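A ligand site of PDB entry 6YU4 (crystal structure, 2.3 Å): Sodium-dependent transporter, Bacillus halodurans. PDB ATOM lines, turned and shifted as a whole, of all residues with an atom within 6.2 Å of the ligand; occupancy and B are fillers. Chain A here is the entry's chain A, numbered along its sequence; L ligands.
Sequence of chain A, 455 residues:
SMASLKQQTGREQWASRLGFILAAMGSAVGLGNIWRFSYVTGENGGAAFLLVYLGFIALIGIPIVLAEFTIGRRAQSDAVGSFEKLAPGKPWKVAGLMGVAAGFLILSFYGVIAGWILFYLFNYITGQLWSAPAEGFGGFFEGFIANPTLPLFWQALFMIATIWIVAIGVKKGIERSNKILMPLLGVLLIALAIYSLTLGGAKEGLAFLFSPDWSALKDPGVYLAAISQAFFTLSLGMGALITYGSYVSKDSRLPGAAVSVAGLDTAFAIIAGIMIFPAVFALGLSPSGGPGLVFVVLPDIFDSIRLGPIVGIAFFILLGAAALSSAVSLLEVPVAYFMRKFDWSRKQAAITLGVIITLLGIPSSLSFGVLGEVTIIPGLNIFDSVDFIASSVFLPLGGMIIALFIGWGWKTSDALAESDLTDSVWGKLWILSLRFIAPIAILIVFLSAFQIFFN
The backbone carbonyl oxygen of Gly 32 is in hydrogen-bond range of the side-chain amide nitrogen of Gln 229, at 2.9 Å. The side-chain hydroxyl (OG) of Ser 235 sits at hydrogen-bond distance from the backbone carbonyl oxygen (O) of Ser 27 (2.6 Å). O of Ala 28 sits close to OD1 of Asp 265. N of Gly 30 is in hydrogen-bond range of OD1 of Asn 33. OG of Ser 329 sits at hydrogen-bond distance from O of Ser 326. The side-chain hydroxyl (OG1) of Thr 233 lies within hydrogen-bond range of the side-chain carboxylate (OD2) of Asp 265 (2.8 Å). The side-chain hydroxyl (OG) of Ser 326 lies within hydrogen-bond range of the backbone carbonyl oxygen (O) of Ser 27 (3.4 Å). The side-chain hydroxyl (OG) of Ser 326 is in hydrogen-bond range of the backbone carbonyl oxygen (O) of Val 29 (3.2 Å).
The side-chain sulfur (SD) of Met 238 lies close to a fluorine (F1) of the ligand, at 2.9 Å. Gly 30 touches the ligand (C to O1, 3.3 Å). OD1 of Asn 33 touches O2 of the ligand, at 3.6 Å. Ala 240 touches the ligand. Ser 326 touches the ligand (O to C5, 3.8 Å). Ser 329 touches the ligand. Leu 330 touches the ligand. Hydrophobic or aromatic side chains within 4 Å of the ligand: Tyr 110, Phe 232, Met 238, Ala 240 and Leu 330.
N of Gly 32 is in hydrogen-bond range of O1 of the ligand (2.7 Å). The backbone NH of Ser 235 sits close to a nitrogen (N1) of the ligand, 3.5 Å away. OG of Ser 235 lies within hydrogen-bond range of N1 of the ligand (2.8 Å). O of Phe 232 is in hydrogen-bond range of N1 of the ligand, 2.9 Å away. The backbone NH (N) of Leu 31 is in hydrogen-bond range of an oxygen (O1) of the ligand, at 3.0 Å. O1 of the ligand lies within hydrogen-bond range of OH of Tyr 110 (3.0 Å). O of Ala 28 sits at hydrogen-bond distance from N1 of the ligand (3.4 Å). A nitrogen (N1) of the ligand lies within hydrogen-bond range of the backbone carbonyl oxygen of Thr 233, 3.4 Å away. The backbone carbonyl oxygen of Ser 27 is in hydrogen-bond range of a nitrogen (N1) of the ligand (3.4 Å).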
ATOM      1  N   SER A  27     -17.472 -19.016   7.982  1.00  0.00           N
ATOM      2  CA  SER A  27     -16.101 -18.979   8.440  1.00  0.00           C
ATOM      3  C   SER A  27     -15.483 -20.369   8.605  1.00  0.00           C
ATOM      4  O   SER A  27     -14.269 -20.513   8.423  1.00  0.00           O
ATOM      5  CB  SER A  27     -16.010 -18.230   9.775  1.00  0.00           C
ATOM      6  OG  SER A  27     -14.743 -18.426  10.372  1.00  0.00           O
ATOM      7  N   ALA A  28     -16.286 -21.374   8.949  1.00  0.00           N
ATOM      8  CA  ALA A  28     -15.748 -22.713   9.151  1.00  0.00           C
ATOM      9  C   ALA A  28     -15.607 -23.481   7.845  1.00  0.00           C
ATOM     10  O   ALA A  28     -14.683 -24.281   7.691  1.00  0.00           O
ATOM     11  CB  ALA A  28     -16.628 -23.502  10.122  1.00  0.00           C
ATOM     12  N   VAL A  29     -16.509 -23.246   6.898  1.00  0.00           N
ATOM     13  CA  VAL A  29     -16.506 -23.973   5.627  1.00  0.00           C
ATOM     14  C   VAL A  29     -15.692 -23.167   4.622  1.00  0.00           C
ATOM     15  O   VAL A  29     -16.096 -22.065   4.221  1.00  0.00           O
ATOM     16  CB  VAL A  29     -17.936 -24.223   5.122  1.00  0.00           C
ATOM     17  CG1 VAL A  29     -17.905 -25.039   3.843  1.00  0.00           C
ATOM     18  CG2 VAL A  29     -18.753 -24.930   6.187  1.00  0.00           C
ATOM     19  N   GLY A  30     -14.553 -23.714   4.201  1.00  0.00           N
ATOM     20  CA  GLY A  30     -13.697 -23.036   3.246  1.00  0.00           C
ATOM     21  C   GLY A  30     -12.618 -23.927   2.661  1.00  0.00           C
ATOM     22  O   GLY A  30     -12.882 -25.072   2.272  1.00  0.00           O
ATOM     23  N   LEU A  31     -11.392 -23.409   2.571  1.00  0.00           N
ATOM     24  CA  LEU A  31     -10.305 -24.173   1.967  1.00  0.00           C
ATOM     25  C   LEU A  31      -9.926 -25.386   2.813  1.00  0.00           C
ATOM     26  O   LEU A  31      -9.517 -26.412   2.267  1.00  0.00           O
ATOM     27  CB  LEU A  31      -9.072 -23.288   1.766  1.00  0.00           C
ATOM     28  CG  LEU A  31      -9.159 -22.171   0.720  1.00  0.00           C
ATOM     29  CD1 LEU A  31      -7.905 -21.329   0.750  1.00  0.00           C
ATOM     30  CD2 LEU A  31      -9.372 -22.763  -0.669  1.00  0.00           C
ATOM     31  N   GLY A  32     -10.069 -25.275   4.137  1.00  0.00           N
ATOM     32  CA  GLY A  32      -9.673 -26.376   5.001  1.00  0.00           C
ATOM     33  C   GLY A  32     -10.466 -27.636   4.772  1.00  0.00           C
ATOM     34  O   GLY A  32      -9.969 -28.743   5.030  1.00  0.00           O
ATOM     35  N   ASN A  33     -11.692 -27.511   4.258  1.00  0.00           N
ATOM     36  CA  ASN A  33     -12.557 -28.669   4.074  1.00  0.00           C
ATOM     37  C   ASN A  33     -12.207 -29.433   2.800  1.00  0.00           C
ATOM     38  O   ASN A  33     -12.275 -30.670   2.781  1.00  0.00           O
ATOM     39  CB  ASN A  33     -14.023 -28.232   4.042  1.00  0.00           C
ATOM     40  CG  ASN A  33     -14.473 -27.616   5.346  1.00  0.00           C
ATOM     41  OD1 ASN A  33     -14.260 -26.424   5.600  1.00  0.00           O
ATOM     42  ND2 ASN A  33     -15.103 -28.423   6.200  1.00  0.00           N
ATOM     43  N   ILE A 106      -1.971 -17.595   9.567  1.00  0.00           N
ATOM     44  CA  ILE A 106      -2.834 -18.436   8.738  1.00  0.00           C
ATOM     45  C   ILE A 106      -3.280 -17.686   7.485  1.00  0.00           C
ATOM     46  O   ILE A 106      -3.145 -18.193   6.370  1.00  0.00           O
ATOM     47  CB  ILE A 106      -4.033 -18.940   9.552  1.00  0.00           C
ATOM     48  CG1 ILE A 106      -3.572 -19.935  10.628  1.00  0.00           C
ATOM     49  CG2 ILE A 106      -5.060 -19.603   8.643  1.00  0.00           C
ATOM     50  CD1 ILE A 106      -4.657 -20.375  11.573  1.00  0.00           C
ATOM     51  N   TYR A 110      -3.046 -18.676   3.749  1.00  0.00           N
ATOM     52  CA  TYR A 110      -4.401 -18.954   3.282  1.00  0.00           C
ATOM     53  C   TYR A 110      -4.720 -18.149   2.022  1.00  0.00           C
ATOM     54  O   TYR A 110      -5.413 -18.644   1.128  1.00  0.00           O
ATOM     55  CB  TYR A 110      -5.412 -18.633   4.386  1.00  0.00           C
ATOM     56  CG  TYR A 110      -6.793 -19.221   4.188  1.00  0.00           C
ATOM     57  CD1 TYR A 110      -7.770 -18.536   3.487  1.00  0.00           C
ATOM     58  CD2 TYR A 110      -7.112 -20.471   4.713  1.00  0.00           C
ATOM     59  CE1 TYR A 110      -9.025 -19.070   3.303  1.00  0.00           C
ATOM     60  CE2 TYR A 110      -8.366 -21.022   4.533  1.00  0.00           C
ATOM     61  CZ  TYR A 110      -9.323 -20.313   3.827  1.00  0.00           C
ATOM     62  OH  TYR A 110     -10.572 -20.854   3.639  1.00  0.00           O
ATOM     63  N   GLN A 229      -5.988 -30.389  12.024  1.00  0.00           N
ATOM     64  CA  GLN A 229      -7.045 -30.274  11.020  1.00  0.00           C
ATOM     65  C   GLN A 229      -8.391 -30.010  11.672  1.00  0.00           C
ATOM     66  O   GLN A 229      -9.228 -29.291  11.118  1.00  0.00           O
ATOM     67  CB  GLN A 229      -7.101 -31.553  10.183  1.00  0.00           C
ATOM     68  CG  GLN A 229      -8.181 -31.548   9.097  1.00  0.00           C
ATOM     69  CD  GLN A 229      -7.975 -30.459   8.074  1.00  0.00           C
ATOM     70  OE1 GLN A 229      -6.841 -30.089   7.749  1.00  0.00           O
ATOM     71  NE2 GLN A 229      -9.071 -29.923   7.549  1.00  0.00           N
ATOM     72  N   PHE A 231      -8.986 -28.346  14.645  1.00  0.00           N
ATOM     73  CA  PHE A 231      -9.000 -26.939  15.033  1.00  0.00           C
ATOM     74  C   PHE A 231      -9.049 -26.033  13.819  1.00  0.00           C
ATOM     75  O   PHE A 231      -9.774 -25.024  13.803  1.00  0.00           O
ATOM     76  CB  PHE A 231      -7.783 -26.613  15.899  1.00  0.00           C
ATOM     77  CG  PHE A 231      -7.992 -26.883  17.363  1.00  0.00           C
ATOM     78  CD1 PHE A 231      -8.634 -25.952  18.164  1.00  0.00           C
ATOM     79  CD2 PHE A 231      -7.521 -28.052  17.932  1.00  0.00           C
ATOM     80  CE1 PHE A 231      -8.824 -26.195  19.514  1.00  0.00           C
ATOM     81  CE2 PHE A 231      -7.705 -28.302  19.278  1.00  0.00           C
ATOM     82  CZ  PHE A 231      -8.355 -27.377  20.078  1.00  0.00           C
ATOM     83  N   PHE A 232      -8.270 -26.364  12.783  1.00  0.00           N
ATOM     84  CA  PHE A 232      -8.214 -25.532  11.584  1.00  0.00           C
ATOM     85  C   PHE A 232      -9.576 -25.427  10.906  1.00  0.00           C
ATOM     86  O   PHE A 232     -10.050 -24.325  10.618  1.00  0.00           O
ATOM     87  CB  PHE A 232      -7.165 -26.092  10.608  1.00  0.00           C
ATOM     88  CG  PHE A 232      -6.931 -25.245   9.396  1.00  0.00           C
ATOM     89  CD1 PHE A 232      -7.801 -25.292   8.309  1.00  0.00           C
ATOM     90  CD2 PHE A 232      -5.830 -24.398   9.319  1.00  0.00           C
ATOM     91  CE1 PHE A 232      -7.582 -24.518   7.193  1.00  0.00           C
ATOM     92  CE2 PHE A 232      -5.604 -23.630   8.199  1.00  0.00           C
ATOM     93  CZ  PHE A 232      -6.484 -23.685   7.134  1.00  0.00           C
ATOM     94  N   THR A 233     -10.212 -26.571  10.643  1.00  0.00           N
ATOM     95  CA  THR A 233     -11.442 -26.583   9.869  1.00  0.00           C
ATOM     96  C   THR A 233     -12.633 -25.981  10.619  1.00  0.00           C
ATOM     97  O   THR A 233     -13.582 -25.544   9.969  1.00  0.00           O
ATOM     98  CB  THR A 233     -11.777 -28.018   9.438  1.00  0.00           C
ATOM     99  OG1 THR A 233     -12.747 -28.007   8.396  1.00  0.00           O
ATOM    100  CG2 THR A 233     -12.324 -28.830  10.612  1.00  0.00           C
ATOM    101  N   LEU A 234     -12.592 -25.939  11.952  1.00  0.00           N
ATOM    102  CA  LEU A 234     -13.669 -25.334  12.733  1.00  0.00           C
ATOM    103  C   LEU A 234     -13.431 -23.859  13.015  1.00  0.00           C
ATOM    104  O   LEU A 234     -14.200 -23.261  13.779  1.00  0.00           O
ATOM    105  CB  LEU A 234     -13.844 -26.083  14.057  1.00  0.00           C
ATOM    106  CG  LEU A 234     -14.374 -27.519  13.964  1.00  0.00           C
ATOM    107  CD1 LEU A 234     -14.539 -28.123  15.343  1.00  0.00           C
ATOM    108  CD2 LEU A 234     -15.690 -27.541  13.194  1.00  0.00           C
ATOM    109  N   SER A 235     -12.405 -23.256  12.410  1.00  0.00           N
ATOM    110  CA  SER A 235     -12.013 -21.876  12.698  1.00  0.00           C
ATOM    111  C   SER A 235     -11.830 -21.671  14.195  1.00  0.00           C
ATOM    112  O   SER A 235     -12.281 -20.679  14.780  1.00  0.00           O
ATOM    113  CB  SER A 235     -13.032 -20.895  12.122  1.00  0.00           C
ATOM    114  OG  SER A 235     -13.333 -21.202  10.775  1.00  0.00           O
ATOM    115  N   LEU A 236     -11.155 -22.627  14.823  1.00  0.00           N
ATOM    116  CA  LEU A 236     -11.166 -22.768  16.272  1.00  0.00           C
ATOM    117  C   LEU A 236      -9.784 -22.477  16.859  1.00  0.00           C
ATOM    118  O   LEU A 236      -8.755 -22.693  16.219  1.00  0.00           O
ATOM    119  CB  LEU A 236     -11.620 -24.179  16.666  1.00  0.00           C
ATOM    120  CG  LEU A 236     -12.066 -24.380  18.110  1.00  0.00           C
ATOM    121  CD1 LEU A 236     -13.073 -23.301  18.501  1.00  0.00           C
ATOM    122  CD2 LEU A 236     -12.665 -25.767  18.304  1.00  0.00           C
ATOM    123  N   MET A 238      -8.354 -19.583  17.859  1.00  0.00           N
ATOM    124  CA  MET A 238      -7.711 -18.289  17.663  1.00  0.00           C
ATOM    125  C   MET A 238      -8.669 -17.114  17.851  1.00  0.00           C
ATOM    126  O   MET A 238      -8.376 -16.009  17.396  1.00  0.00           O
ATOM    127  CB  MET A 238      -7.063 -18.215  16.278  1.00  0.00           C
ATOM    128  CG  MET A 238      -7.993 -18.531  15.133  1.00  0.00           C
ATOM    129  SD  MET A 238      -7.322 -18.004  13.546  1.00  0.00           S
ATOM    130  CE  MET A 238      -7.701 -16.251  13.602  1.00  0.00           C
ATOM    131  N   GLY A 239      -9.796 -17.333  18.518  1.00  0.00           N
ATOM    132  CA  GLY A 239     -10.708 -16.253  18.812  1.00  0.00           C
ATOM    133  C   GLY A 239     -11.528 -15.748  17.656  1.00  0.00           C
ATOM    134  O   GLY A 239     -12.198 -14.720  17.800  1.00  0.00           O
ATOM    135  N   ALA A 240     -11.492 -16.425  16.507  1.00  0.00           N
ATOM    136  CA  ALA A 240     -12.346 -16.038  15.389  1.00  0.00           C
ATOM    137  C   ALA A 240     -13.826 -16.194  15.731  1.00  0.00           C
ATOM    138  O   ALA A 240     -14.651 -15.353  15.376  1.00  0.00           O
ATOM    139  CB  ALA A 240     -12.002 -16.846  14.154  1.00  0.00           C
ATOM    140  N   LEU A 241     -14.169 -17.278  16.425  1.00  0.00           N
ATOM    141  CA  LEU A 241     -15.533 -17.460  16.896  1.00  0.00           C
ATOM    142  C   LEU A 241     -15.815 -16.648  18.152  1.00  0.00           C
ATOM    143  O   LEU A 241     -16.979 -16.367  18.442  1.00  0.00           O
ATOM    144  CB  LEU A 241     -15.808 -18.943  17.145  1.00  0.00           C
ATOM    145  CG  LEU A 241     -15.498 -19.839  15.949  1.00  0.00           C
ATOM    146  CD1 LEU A 241     -15.790 -21.310  16.250  1.00  0.00           C
ATOM    147  CD2 LEU A 241     -16.262 -19.369  14.712  1.00  0.00           C
ATOM    148  N   ASP A 265     -19.840 -28.391   8.792  1.00  0.00           N
ATOM    149  CA  ASP A 265     -18.444 -28.340   8.361  1.00  0.00           C
ATOM    150  C   ASP A 265     -17.883 -29.744   8.128  1.00  0.00           C
ATOM    151  O   ASP A 265     -17.096 -29.964   7.200  1.00  0.00           O
ATOM    152  CB  ASP A 265     -17.601 -27.598   9.396  1.00  0.00           C
ATOM    153  CG  ASP A 265     -16.137 -27.507   9.010  1.00  0.00           C
ATOM    154  OD1 ASP A 265     -15.766 -26.516   8.339  1.00  0.00           O
ATOM    155  OD2 ASP A 265     -15.375 -28.428   9.370  1.00  0.00           O
ATOM    156  N   ALA A 322     -16.232 -19.558  -0.722  1.00  0.00           N
ATOM    157  CA  ALA A 322     -16.053 -20.146   0.609  1.00  0.00           C
ATOM    158  C   ALA A 322     -14.739 -19.709   1.224  1.00  0.00           C
ATOM    159  O   ALA A 322     -14.688 -19.390   2.422  1.00  0.00           O
ATOM    160  CB  ALA A 322     -16.140 -21.664   0.518  1.00  0.00           C
ATOM    161  N   SER A 326     -14.081 -17.230   4.622  1.00  0.00           N
ATOM    162  CA  SER A 326     -13.199 -17.741   5.663  1.00  0.00           C
ATOM    163  C   SER A 326     -12.048 -16.776   5.928  1.00  0.00           C
ATOM    164  O   SER A 326     -11.686 -16.538   7.081  1.00  0.00           O
ATOM    165  CB  SER A 326     -12.652 -19.121   5.267  1.00  0.00           C
ATOM    166  OG  SER A 326     -13.706 -20.057   5.090  1.00  0.00           O
ATOM    167  N   ALA A 327     -11.472 -16.208   4.873  1.00  0.00           N
ATOM    168  CA  ALA A 327     -10.406 -15.224   5.043  1.00  0.00           C
ATOM    169  C   ALA A 327     -10.912 -13.962   5.724  1.00  0.00           C
ATOM    170  O   ALA A 327     -10.167 -13.323   6.467  1.00  0.00           O
ATOM    171  CB  ALA A 327      -9.792 -14.877   3.684  1.00  0.00           C
ATOM    172  N   SER A 329     -13.167 -13.765   8.129  1.00  0.00           N
ATOM    173  CA  SER A 329     -13.128 -14.019   9.566  1.00  0.00           C
ATOM    174  C   SER A 329     -11.706 -14.106  10.084  1.00  0.00           C
ATOM    175  O   SER A 329     -11.452 -13.781  11.250  1.00  0.00           O
ATOM    176  CB  SER A 329     -13.900 -15.297   9.906  1.00  0.00           C
ATOM    177  OG  SER A 329     -13.126 -16.447   9.604  1.00  0.00           O
ATOM    178  N   LEU A 330     -10.767 -14.537   9.248  1.00  0.00           N
ATOM    179  CA  LEU A 330      -9.362 -14.511   9.628  1.00  0.00           C
ATOM    180  C   LEU A 330      -8.887 -13.076   9.831  1.00  0.00           C
ATOM    181  O   LEU A 330      -8.294 -12.745  10.860  1.00  0.00           O
ATOM    182  CB  LEU A 330      -8.510 -15.217   8.573  1.00  0.00           C
ATOM    183  CG  LEU A 330      -8.452 -16.735   8.614  1.00  0.00           C
ATOM    184  CD1 LEU A 330      -7.946 -17.307   7.304  1.00  0.00           C
ATOM    185  CD2 LEU A 330      -7.568 -17.176   9.770  1.00  0.00           C
ATOM    186  N   VAL A 333     -10.128 -10.919  12.963  1.00  0.00           N
ATOM    187  CA  VAL A 333      -9.611 -11.208  14.303  1.00  0.00           C
ATOM    188  C   VAL A 333      -8.565 -10.178  14.716  1.00  0.00           C
ATOM    189  O   VAL A 333      -8.732  -9.536  15.759  1.00  0.00           O
ATOM    190  CB  VAL A 333      -9.067 -12.640  14.392  1.00  0.00           C
ATOM    191  CG1 VAL A 333      -8.444 -12.885  15.758  1.00  0.00           C
ATOM    192  CG2 VAL A 333     -10.167 -13.618  14.132  1.00  0.00           C
ATOM    193  N   LEU A 395      -3.015 -22.891  17.396  1.00  0.00           N
ATOM    194  CA  LEU A 395      -4.438 -23.241  17.420  1.00  0.00           C
ATOM    195  C   LEU A 395      -4.774 -24.243  18.517  1.00  0.00           C
ATOM    196  O   LEU A 395      -5.754 -24.006  19.253  1.00  0.00           O
ATOM    197  CB  LEU A 395      -4.880 -23.762  16.043  1.00  0.00           C
ATOM    198  CG  LEU A 395      -5.092 -22.750  14.917  1.00  0.00           C
ATOM    199  CD1 LEU A 395      -6.022 -23.319  13.859  1.00  0.00           C
ATOM    200  CD2 LEU A 395      -5.634 -21.444  15.470  1.00  0.00           C
HETATM  201  N1  LIG L   1     -11.891 -22.812   9.018  1.00  0.00           N
HETATM  202  C1  LIG L   1     -11.398 -22.315   7.744  1.00  0.00           C
HETATM  203  C2  LIG L   1     -11.318 -23.448   6.736  1.00  0.00           C
HETATM  204  O1  LIG L   1     -11.061 -23.195   5.529  1.00  0.00           O
HETATM  205  O2  LIG L   1     -11.516 -24.643   7.092  1.00  0.00           O
HETATM  206  C3  LIG L   1     -10.017 -21.663   7.913  1.00  0.00           C
HETATM  207  C4  LIG L   1     -10.007 -20.731   9.118  1.00  0.00           C
HETATM  208  C5  LIG L   1     -10.811 -19.597   9.147  1.00  0.00           C
HETATM  209  C6  LIG L   1      -9.191 -21.027  10.203  1.00  0.00           C
HETATM  210  C7  LIG L   1     -10.794 -18.762  10.247  1.00  0.00           C
HETATM  211  C8  LIG L   1      -9.167 -20.186  11.305  1.00  0.00           C
HETATM  212  C9  LIG L   1      -9.973 -19.048  11.324  1.00  0.00           C
HETATM  213  F1  LIG L   1      -9.950 -18.233  12.415  1.00  0.00           F
